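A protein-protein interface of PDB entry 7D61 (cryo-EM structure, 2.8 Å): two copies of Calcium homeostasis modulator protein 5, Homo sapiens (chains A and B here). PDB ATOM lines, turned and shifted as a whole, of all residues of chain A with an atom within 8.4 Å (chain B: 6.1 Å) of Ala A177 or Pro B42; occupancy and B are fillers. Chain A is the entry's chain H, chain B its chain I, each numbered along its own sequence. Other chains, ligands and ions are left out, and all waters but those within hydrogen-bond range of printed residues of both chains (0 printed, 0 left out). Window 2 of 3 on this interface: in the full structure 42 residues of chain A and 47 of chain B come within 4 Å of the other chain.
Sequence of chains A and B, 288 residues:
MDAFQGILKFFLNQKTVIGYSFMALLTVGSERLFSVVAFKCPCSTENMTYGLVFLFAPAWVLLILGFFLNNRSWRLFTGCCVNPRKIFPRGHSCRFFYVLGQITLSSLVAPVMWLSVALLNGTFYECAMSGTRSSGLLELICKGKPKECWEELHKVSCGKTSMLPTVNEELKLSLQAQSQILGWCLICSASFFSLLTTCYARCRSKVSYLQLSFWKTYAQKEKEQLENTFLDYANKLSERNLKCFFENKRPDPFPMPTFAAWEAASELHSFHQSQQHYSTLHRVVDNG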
ATOM      1  N   LEU A 119      13.059  33.692  10.315  1.00  0.00           N
ATOM      2  CA  LEU A 119      13.080  33.579   8.864  1.00  0.00           C
ATOM      3  C   LEU A 119      13.718  32.285   8.375  1.00  0.00           C
ATOM      4  O   LEU A 119      13.459  31.880   7.239  1.00  0.00           O
ATOM      5  CB  LEU A 119      13.812  34.771   8.246  1.00  0.00           C
ATOM      6  CG  LEU A 119      13.005  36.061   8.112  1.00  0.00           C
ATOM      7  CD1 LEU A 119      13.886  37.198   7.627  1.00  0.00           C
ATOM      8  CD2 LEU A 119      11.831  35.863   7.183  1.00  0.00           C
ATOM      9  N   GLY A 122      10.457  28.982   7.947  1.00  0.00           N
ATOM     10  CA  GLY A 122       9.600  29.799   7.110  1.00  0.00           C
ATOM     11  C   GLY A 122       8.104  29.612   7.262  1.00  0.00           C
ATOM     12  O   GLY A 122       7.407  29.372   6.274  1.00  0.00           O
ATOM     13  N   TYR A 125       6.672  33.901   7.238  1.00  0.00           N
ATOM     14  CA  TYR A 125       6.740  34.568   5.945  1.00  0.00           C
ATOM     15  C   TYR A 125       5.755  33.970   4.952  1.00  0.00           C
ATOM     16  O   TYR A 125       5.235  34.691   4.095  1.00  0.00           O
ATOM     17  CB  TYR A 125       8.175  34.492   5.412  1.00  0.00           C
ATOM     18  CG  TYR A 125       8.418  35.041   4.018  1.00  0.00           C
ATOM     19  CD1 TYR A 125       8.742  36.377   3.829  1.00  0.00           C
ATOM     20  CD2 TYR A 125       8.384  34.211   2.900  1.00  0.00           C
ATOM     21  CE1 TYR A 125       8.984  36.878   2.566  1.00  0.00           C
ATOM     22  CE2 TYR A 125       8.619  34.705   1.636  1.00  0.00           C
ATOM     23  CZ  TYR A 125       8.920  36.038   1.476  1.00  0.00           C
ATOM     24  OH  TYR A 125       9.161  36.533   0.218  1.00  0.00           O
ATOM     25  N   GLU A 126       5.497  32.664   5.049  1.00  0.00           N
ATOM     26  CA  GLU A 126       4.576  32.006   4.128  1.00  0.00           C
ATOM     27  C   GLU A 126       3.138  32.452   4.371  1.00  0.00           C
ATOM     28  O   GLU A 126       2.378  32.669   3.420  1.00  0.00           O
ATOM     29  CB  GLU A 126       4.725  30.489   4.266  1.00  0.00           C
ATOM     30  CG  GLU A 126       3.534  29.661   3.828  1.00  0.00           C
ATOM     31  CD  GLU A 126       3.589  28.249   4.368  1.00  0.00           C
ATOM     32  OE1 GLU A 126       4.702  27.691   4.459  1.00  0.00           O
ATOM     33  OE2 GLU A 126       2.521  27.695   4.704  1.00  0.00           O
ATOM     34  N   GLU A 169       1.334  21.950  -3.034  1.00  0.00           N
ATOM     35  CA  GLU A 169       2.511  21.489  -2.315  1.00  0.00           C
ATOM     36  C   GLU A 169       3.807  22.026  -2.911  1.00  0.00           C
ATOM     37  O   GLU A 169       4.837  22.010  -2.230  1.00  0.00           O
ATOM     38  CB  GLU A 169       2.539  19.954  -2.285  1.00  0.00           C
ATOM     39  CG  GLU A 169       3.337  19.345  -1.136  1.00  0.00           C
ATOM     40  CD  GLU A 169       2.804  19.739   0.230  1.00  0.00           C
ATOM     41  OE1 GLU A 169       1.567  19.835   0.392  1.00  0.00           O
ATOM     42  OE2 GLU A 169       3.623  19.957   1.148  1.00  0.00           O
ATOM     43  N   GLU A 170       3.781  22.521  -4.145  1.00  0.00           N
ATOM     44  CA  GLU A 170       4.941  23.173  -4.733  1.00  0.00           C
ATOM     45  C   GLU A 170       4.816  24.690  -4.740  1.00  0.00           C
ATOM     46  O   GLU A 170       5.751  25.374  -5.166  1.00  0.00           O
ATOM     47  CB  GLU A 170       5.193  22.645  -6.153  1.00  0.00           C
ATOM     48  CG  GLU A 170       4.076  22.880  -7.161  1.00  0.00           C
ATOM     49  CD  GLU A 170       4.242  24.165  -7.952  1.00  0.00           C
ATOM     50  OE1 GLU A 170       5.374  24.686  -8.019  1.00  0.00           O
ATOM     51  OE2 GLU A 170       3.238  24.655  -8.502  1.00  0.00           O
ATOM     52  N   LEU A 171       3.685  25.230  -4.289  1.00  0.00           N
ATOM     53  CA  LEU A 171       3.589  26.649  -3.979  1.00  0.00           C
ATOM     54  C   LEU A 171       3.939  26.943  -2.532  1.00  0.00           C
ATOM     55  O   LEU A 171       4.228  28.096  -2.197  1.00  0.00           O
ATOM     56  CB  LEU A 171       2.182  27.177  -4.271  1.00  0.00           C
ATOM     57  CG  LEU A 171       1.900  27.666  -5.690  1.00  0.00           C
ATOM     58  CD1 LEU A 171       0.435  28.028  -5.839  1.00  0.00           C
ATOM     59  CD2 LEU A 171       2.781  28.853  -6.024  1.00  0.00           C
ATOM     60  N   LYS A 172       3.909  25.927  -1.670  1.00  0.00           N
ATOM     61  CA  LYS A 172       4.389  26.081  -0.305  1.00  0.00           C
ATOM     62  C   LYS A 172       5.908  26.008  -0.245  1.00  0.00           C
ATOM     63  O   LYS A 172       6.535  26.737   0.528  1.00  0.00           O
ATOM     64  CB  LYS A 172       3.772  25.010   0.592  1.00  0.00           C
ATOM     65  CG  LYS A 172       2.351  25.310   1.025  1.00  0.00           C
ATOM     66  CD  LYS A 172       1.826  24.240   1.968  1.00  0.00           C
ATOM     67  CE  LYS A 172       2.701  24.107   3.204  1.00  0.00           C
ATOM     68  NZ  LYS A 172       1.985  23.420   4.312  1.00  0.00           N
ATOM     69  N   LEU A 173       6.511  25.133  -1.054  1.00  0.00           N
ATOM     70  CA  LEU A 173       7.963  24.987  -1.056  1.00  0.00           C
ATOM     71  C   LEU A 173       8.654  26.178  -1.704  1.00  0.00           C
ATOM     72  O   LEU A 173       9.826  26.438  -1.421  1.00  0.00           O
ATOM     73  CB  LEU A 173       8.359  23.699  -1.775  1.00  0.00           C
ATOM     74  CG  LEU A 173       8.079  22.381  -1.054  1.00  0.00           C
ATOM     75  CD1 LEU A 173       8.314  21.215  -1.995  1.00  0.00           C
ATOM     76  CD2 LEU A 173       8.941  22.253   0.187  1.00  0.00           C
ATOM     77  N   SER A 174       7.957  26.904  -2.576  1.00  0.00           N
ATOM     78  CA  SER A 174       8.537  28.086  -3.193  1.00  0.00           C
ATOM     79  C   SER A 174       8.494  29.302  -2.279  1.00  0.00           C
ATOM     80  O   SER A 174       9.285  30.232  -2.470  1.00  0.00           O
ATOM     81  CB  SER A 174       7.815  28.402  -4.503  1.00  0.00           C
ATOM     82  OG  SER A 174       8.331  29.579  -5.098  1.00  0.00           O
ATOM     83  N   LEU A 175       7.593  29.317  -1.298  1.00  0.00           N
ATOM     84  CA  LEU A 175       7.538  30.386  -0.312  1.00  0.00           C
ATOM     85  C   LEU A 175       8.315  30.063   0.955  1.00  0.00           C
ATOM     86  O   LEU A 175       8.776  30.986   1.633  1.00  0.00           O
ATOM     87  CB  LEU A 175       6.082  30.699   0.055  1.00  0.00           C
ATOM     88  CG  LEU A 175       5.261  31.444  -0.995  1.00  0.00           C
ATOM     89  CD1 LEU A 175       3.802  31.485  -0.591  1.00  0.00           C
ATOM     90  CD2 LEU A 175       5.795  32.847  -1.202  1.00  0.00           C
ATOM     91  N   GLN A 176       8.476  28.783   1.283  1.00  0.00           N
ATOM     92  CA  GLN A 176       9.302  28.355   2.405  1.00  0.00           C
ATOM     93  C   GLN A 176      10.789  28.370   2.070  1.00  0.00           C
ATOM     94  O   GLN A 176      11.612  28.108   2.952  1.00  0.00           O
ATOM     95  CB  GLN A 176       8.873  26.952   2.848  1.00  0.00           C
ATOM     96  CG  GLN A 176       9.044  26.647   4.327  1.00  0.00           C
ATOM     97  CD  GLN A 176      10.251  25.777   4.609  1.00  0.00           C
ATOM     98  OE1 GLN A 176      10.688  25.006   3.756  1.00  0.00           O
ATOM     99  NE2 GLN A 176      10.793  25.892   5.816  1.00  0.00           N
ATOM    100  N   ALA A 177      11.153  28.683   0.827  1.00  0.00           N
ATOM    101  CA  ALA A 177      12.542  28.798   0.422  1.00  0.00           C
ATOM    102  C   ALA A 177      12.956  30.222   0.092  1.00  0.00           C
ATOM    103  O   ALA A 177      14.158  30.485  -0.014  1.00  0.00           O
ATOM    104  CB  ALA A 177      12.824  27.903  -0.793  1.00  0.00           C
ATOM    105  N   GLN A 178      12.008  31.142  -0.076  1.00  0.00           N
ATOM    106  CA  GLN A 178      12.345  32.550  -0.235  1.00  0.00           C
ATOM    107  C   GLN A 178      12.613  33.233   1.097  1.00  0.00           C
ATOM    108  O   GLN A 178      13.216  34.310   1.114  1.00  0.00           O
ATOM    109  CB  GLN A 178      11.225  33.288  -0.966  1.00  0.00           C
ATOM    110  CG  GLN A 178      11.186  33.047  -2.459  1.00  0.00           C
ATOM    111  CD  GLN A 178      10.093  33.839  -3.144  1.00  0.00           C
ATOM    112  OE1 GLN A 178       9.238  34.431  -2.488  1.00  0.00           O
ATOM    113  NE2 GLN A 178      10.114  33.853  -4.470  1.00  0.00           N
ATOM    114  N   SER A 179      12.175  32.637   2.204  1.00  0.00           N
ATOM    115  CA  SER A 179      12.454  33.180   3.524  1.00  0.00           C
ATOM    116  C   SER A 179      13.773  32.685   4.091  1.00  0.00           C
ATOM    117  O   SER A 179      14.424  33.414   4.846  1.00  0.00           O
ATOM    118  CB  SER A 179      11.327  32.824   4.494  1.00  0.00           C
ATOM    119  OG  SER A 179      11.270  31.429   4.712  1.00  0.00           O
ATOM    120  N   GLN A 180      14.180  31.462   3.750  1.00  0.00           N
ATOM    121  CA  GLN A 180      15.468  30.958   4.203  1.00  0.00           C
ATOM    122  C   GLN A 180      16.627  31.584   3.441  1.00  0.00           C
ATOM    123  O   GLN A 180      17.731  31.668   3.982  1.00  0.00           O
ATOM    124  CB  GLN A 180      15.504  29.436   4.083  1.00  0.00           C
ATOM    125  CG  GLN A 180      14.550  28.739   5.033  1.00  0.00           C
ATOM    126  CD  GLN A 180      14.565  27.235   4.885  1.00  0.00           C
ATOM    127  OE1 GLN A 180      14.625  26.712   3.775  1.00  0.00           O
ATOM    128  NE2 GLN A 180      14.507  26.530   6.005  1.00  0.00           N
ATOM    129  N   ILE A 181      16.401  32.028   2.204  1.00  0.00           N
ATOM    130  CA  ILE A 181      17.405  32.821   1.504  1.00  0.00           C
ATOM    131  C   ILE A 181      17.520  34.200   2.142  1.00  0.00           C
ATOM    132  O   ILE A 181      18.625  34.715   2.353  1.00  0.00           O
ATOM    133  CB  ILE A 181      17.059  32.899   0.003  1.00  0.00           C
ATOM    134  CG1 ILE A 181      17.318  31.552  -0.669  1.00  0.00           C
ATOM    135  CG2 ILE A 181      17.850  33.989  -0.706  1.00  0.00           C
ATOM    136  CD1 ILE A 181      16.736  31.444  -2.054  1.00  0.00           C
ATOM    137  N   LEU A 182      16.382  34.801   2.499  1.00  0.00           N
ATOM    138  CA  LEU A 182      16.379  36.091   3.180  1.00  0.00           C
ATOM    139  C   LEU A 182      16.896  36.000   4.608  1.00  0.00           C
ATOM    140  O   LEU A 182      17.378  37.003   5.141  1.00  0.00           O
ATOM    141  CB  LEU A 182      14.970  36.678   3.193  1.00  0.00           C
ATOM    142  CG  LEU A 182      14.581  37.596   2.040  1.00  0.00           C
ATOM    143  CD1 LEU A 182      13.147  38.054   2.209  1.00  0.00           C
ATOM    144  CD2 LEU A 182      15.519  38.783   1.972  1.00  0.00           C
ATOM    145  N   GLY A 183      16.788  34.831   5.241  1.00  0.00           N
ATOM    146  CA  GLY A 183      17.310  34.679   6.588  1.00  0.00           C
ATOM    147  C   GLY A 183      18.826  34.671   6.632  1.00  0.00           C
ATOM    148  O   GLY A 183      19.429  35.214   7.559  1.00  0.00           O
ATOM    149  N   TRP A 184      19.463  34.062   5.629  1.00  0.00           N
ATOM    150  CA  TRP A 184      20.920  34.045   5.577  1.00  0.00           C
ATOM    151  C   TRP A 184      21.499  35.366   5.099  1.00  0.00           C
ATOM    152  O   TRP A 184      22.664  35.654   5.385  1.00  0.00           O
ATOM    153  CB  TRP A 184      21.415  32.923   4.666  1.00  0.00           C
ATOM    154  CG  TRP A 184      21.313  31.549   5.248  1.00  0.00           C
ATOM    155  CD1 TRP A 184      20.530  30.532   4.800  1.00  0.00           C
ATOM    156  CD2 TRP A 184      22.040  31.029   6.368  1.00  0.00           C
ATOM    157  NE1 TRP A 184      20.706  29.417   5.576  1.00  0.00           N
ATOM    158  CE2 TRP A 184      21.630  29.695   6.546  1.00  0.00           C
ATOM    159  CE3 TRP A 184      22.992  31.563   7.242  1.00  0.00           C
ATOM    160  CZ2 TRP A 184      22.136  28.888   7.559  1.00  0.00           C
ATOM    161  CZ3 TRP A 184      23.492  30.761   8.247  1.00  0.00           C
ATOM    162  CH2 TRP A 184      23.064  29.438   8.398  1.00  0.00           C
ATOM    163  N   LYS B  40      15.051  21.558   2.710  1.00  0.00           N
ATOM    164  CA  LYS B  40      14.150  20.797   1.852  1.00  0.00           C
ATOM    165  C   LYS B  40      14.133  21.468   0.487  1.00  0.00           C
ATOM    166  O   LYS B  40      13.706  22.619   0.355  1.00  0.00           O
ATOM    167  CB  LYS B  40      12.744  20.685   2.459  1.00  0.00           C
ATOM    168  CG  LYS B  40      12.193  21.943   3.114  1.00  0.00           C
ATOM    169  CD  LYS B  40      10.882  21.655   3.826  1.00  0.00           C
ATOM    170  CE  LYS B  40      11.110  20.846   5.094  1.00  0.00           C
ATOM    171  NZ  LYS B  40      11.854  21.624   6.124  1.00  0.00           N
ATOM    172  N   CYS B  41      14.633  20.756  -0.513  1.00  0.00           N
ATOM    173  CA  CYS B  41      14.908  21.363  -1.810  1.00  0.00           C
ATOM    174  C   CYS B  41      13.613  21.620  -2.571  1.00  0.00           C
ATOM    175  O   CYS B  41      12.834  20.686  -2.792  1.00  0.00           O
ATOM    176  CB  CYS B  41      15.831  20.450  -2.620  1.00  0.00           C
ATOM    177  SG  CYS B  41      16.275  21.033  -4.274  1.00  0.00           S
ATOM    178  N   PRO B  42      13.343  22.856  -2.978  1.00  0.00           N
ATOM    179  CA  PRO B  42      12.216  23.104  -3.877  1.00  0.00           C
ATOM    180  C   PRO B  42      12.563  22.674  -5.291  1.00  0.00           C
ATOM    181  O   PRO B  42      13.714  22.729  -5.722  1.00  0.00           O
ATOM    182  CB  PRO B  42      12.027  24.622  -3.791  1.00  0.00           C
ATOM    183  CG  PRO B  42      13.395  25.137  -3.522  1.00  0.00           C
ATOM    184  CD  PRO B  42      14.094  24.089  -2.688  1.00  0.00           C
ATOM    185  N   CYS B  43      11.550  22.212  -6.011  1.00  0.00           N
ATOM    186  CA  CYS B  43      11.743  21.780  -7.389  1.00  0.00           C
ATOM    187  C   CYS B  43      11.279  22.910  -8.302  1.00  0.00           C
ATOM    188  O   CYS B  43      10.213  22.863  -8.914  1.00  0.00           O
ATOM    189  CB  CYS B  43      11.009  20.469  -7.631  1.00  0.00           C
ATOM    190  SG  CYS B  43      11.954  19.041  -7.032  1.00  0.00           S
ATOM    191  N   SER B  44      12.112  23.946  -8.391  1.00  0.00           N
ATOM    192  CA  SER B  44      11.752  25.188  -9.066  1.00  0.00           C
ATOM    193  C   SER B  44      12.967  25.701  -9.829  1.00  0.00           C
ATOM    194  O   SER B  44      13.960  24.991 -10.010  1.00  0.00           O
ATOM    195  CB  SER B  44      11.244  26.230  -8.061  1.00  0.00           C
ATOM    196  OG  SER B  44      10.249  25.688  -7.209  1.00  0.00           O
ATOM    197  N   GLU B  46      14.599  28.406  -8.745  1.00  0.00           N
ATOM    198  CA  GLU B  46      15.496  28.945  -7.732  1.00  0.00           C
ATOM    199  C   GLU B  46      16.382  27.871  -7.117  1.00  0.00           C
ATOM    200  O   GLU B  46      16.792  27.997  -5.958  1.00  0.00           O
ATOM    201  CB  GLU B  46      14.691  29.657  -6.645  1.00  0.00           C
ATOM    202  CG  GLU B  46      13.526  28.847  -6.113  1.00  0.00           C
ATOM    203  CD  GLU B  46      12.929  29.441  -4.854  1.00  0.00           C
ATOM    204  OE1 GLU B  46      11.802  29.974  -4.921  1.00  0.00           O
ATOM    205  OE2 GLU B  46      13.588  29.375  -3.795  1.00  0.00           O
ATOM    206  N   ASN B  47      16.668  26.807  -7.872  1.00  0.00           N
ATOM    207  CA  ASN B  47      17.480  25.705  -7.368  1.00  0.00           C
ATOM    208  C   ASN B  47      18.930  26.115  -7.177  1.00  0.00           C
ATOM    209  O   ASN B  47      19.578  25.686  -6.215  1.00  0.00           O
ATOM    210  CB  ASN B  47      17.394  24.521  -8.328  1.00  0.00           C
ATOM    211  CG  ASN B  47      16.403  23.488  -7.881  1.00  0.00           C
ATOM    212  OD1 ASN B  47      16.341  23.156  -6.709  1.00  0.00           O
ATOM    213  ND2 ASN B  47      15.624  22.968  -8.813  1.00  0.00           N
ATOM    214  N   TYR B  50      19.284  28.537  -4.023  1.00  0.00           N
ATOM    215  CA  TYR B  50      18.932  27.975  -2.722  1.00  0.00           C
ATOM    216  C   TYR B  50      19.996  27.004  -2.221  1.00  0.00           C
ATOM    217  O   TYR B  50      20.278  26.952  -1.020  1.00  0.00           O
ATOM    218  CB  TYR B  50      17.570  27.289  -2.809  1.00  0.00           C
ATOM    219  CG  TYR B  50      17.071  26.710  -1.510  1.00  0.00           C
ATOM    220  CD1 TYR B  50      17.133  25.347  -1.268  1.00  0.00           C
ATOM    221  CD2 TYR B  50      16.522  27.522  -0.531  1.00  0.00           C
ATOM    222  CE1 TYR B  50      16.669  24.810  -0.088  1.00  0.00           C
ATOM    223  CE2 TYR B  50      16.058  26.994   0.657  1.00  0.00           C
ATOM    224  CZ  TYR B  50      16.133  25.637   0.870  1.00  0.00           C
ATOM    225  OH  TYR B  50      15.674  25.098   2.047  1.00  0.00           O
ATOM    226  N   CYS B 127      20.873  19.603  -5.093  1.00  0.00           N
ATOM    227  CA  CYS B 127      19.851  20.621  -5.314  1.00  0.00           C
ATOM    228  C   CYS B 127      20.380  21.780  -6.153  1.00  0.00           C
ATOM    229  O   CYS B 127      19.616  22.399  -6.899  1.00  0.00           O
ATOM    230  CB  CYS B 127      19.328  21.122  -3.965  1.00  0.00           C
ATOM    231  SG  CYS B 127      17.898  22.235  -4.014  1.00  0.00           S
ATOM    232  N   HIS B 154      15.627  19.654 -13.057  1.00  0.00           N
ATOM    233  CA  HIS B 154      15.505  20.349 -11.780  1.00  0.00           C
ATOM    234  C   HIS B 154      14.353  19.849 -10.916  1.00  0.00           C
ATOM    235  O   HIS B 154      14.091  20.444  -9.867  1.00  0.00           O
ATOM    236  CB  HIS B 154      15.369  21.860 -12.011  1.00  0.00           C
ATOM    237  CG  HIS B 154      14.193  22.253 -12.851  1.00  0.00           C
ATOM    238  ND1 HIS B 154      14.327  22.709 -14.144  1.00  0.00           N
ATOM    239  CD2 HIS B 154      12.868  22.296 -12.573  1.00  0.00           C
ATOM    240  CE1 HIS B 154      13.134  22.995 -14.634  1.00  0.00           C
ATOM    241  NE2 HIS B 154      12.232  22.752 -13.701  1.00  0.00           N
ATOM    242  N   SER B 157      14.869  15.882  -7.471  1.00  0.00           N
ATOM    243  CA  SER B 157      14.980  15.715  -6.027  1.00  0.00           C
ATOM    244  C   SER B 157      13.637  15.372  -5.393  1.00  0.00           C
ATOM    245  O   SER B 157      13.573  14.543  -4.479  1.00  0.00           O
ATOM    246  CB  SER B 157      15.556  16.982  -5.398  1.00  0.00           C
ATOM    247  OG  SER B 157      16.667  17.457  -6.138  1.00  0.00           O
ATOM    248  N   CYS B 158      12.558  15.997  -5.864  1.00  0.00           N
ATOM    249  CA  CYS B 158      11.229  15.759  -5.314  1.00  0.00           C
ATOM    250  C   CYS B 158      10.531  14.554  -5.930  1.00  0.00           C
ATOM    251  O   CYS B 158       9.400  14.250  -5.536  1.00  0.00           O
ATOM    252  CB  CYS B 158      10.344  16.993  -5.514  1.00  0.00           C
ATOM    253  SG  CYS B 158      11.154  18.580  -5.224  1.00  0.00           S
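The side-chain carboxylate (OE1) of Glu B46 is in hydrogen-bond range of the side-chain hydroxyl (OG) of Ser A174.
The side-chain hydroxyl (OH) of Tyr B50 is in hydrogen-bond range of the side-chain amide oxygen (OE1) of Gln A180, 2.6 Å away.
The side-chain amide oxygen of Gln A178 is in hydrogen-bond range of the side-chain hydroxyl of Tyr A125 (3.4 Å).
The side-chain amide oxygen (OE1) of Gln A180 lies close to the backbone carbonyl oxygen (O) of Gln A176 (3.4 Å).
O of Pro B42 sits close to OD1 of Asn B47 (2.8 Å).
SG of Cys B127 forms a disulfide with SG of Cys B41 (2.0 Å).
The side-chain sulfur of Cys B43 is disulfide-bonded to the side-chain sulfur of Cys B158, 2.0 Å away.
Among the printed residues, pairs that only touch across the chains: Gln A176 with Lys B40, Ala A177 with Glu B46, Ala A177 with Tyr B50, Leu A173 with Pro B42, Ala A177 with Pro B42 and Gln A178 with Glu B46.
No position is printed for both chains.
Of the 8 pairs that touch across the chains among the printed residues, none has its exchanged pair printed and touching as well.
Printed residues of chain B that touch a printed residue of chain A: Lys B40, Pro B42, Glu B46 and Tyr B50.
Hydrophobic or aromatic side chains of chain B that line the printed part of chain A: Pro B42 and Tyr B50.
Of the 20 printed residues of chain A, 6 touch a printed residue of chain B.
Among the printed residues, no Asp or Glu carboxylate lies within 4 Å of a Lys or Arg side-chain nitrogen of the other chain.
Of the printed residues of chain B, Leu A173 touches Pro B42 (3.7 Å).
Printed residues of chain B within 4 Å of Ser A174: Glu B46.
Of the printed residues of chain B, Gln A178 touches Glu B46.
Of the printed residues of chain A, Lys B40 touches Gln A176 (3.4 Å).
No residue of chain A comes within 4 Å of Cys B41.
No residue of chain A comes within 4 Å of Cys B43.
Printed residues of chain A within 4 Å of Tyr B50: Ala A177 and Gln A180.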
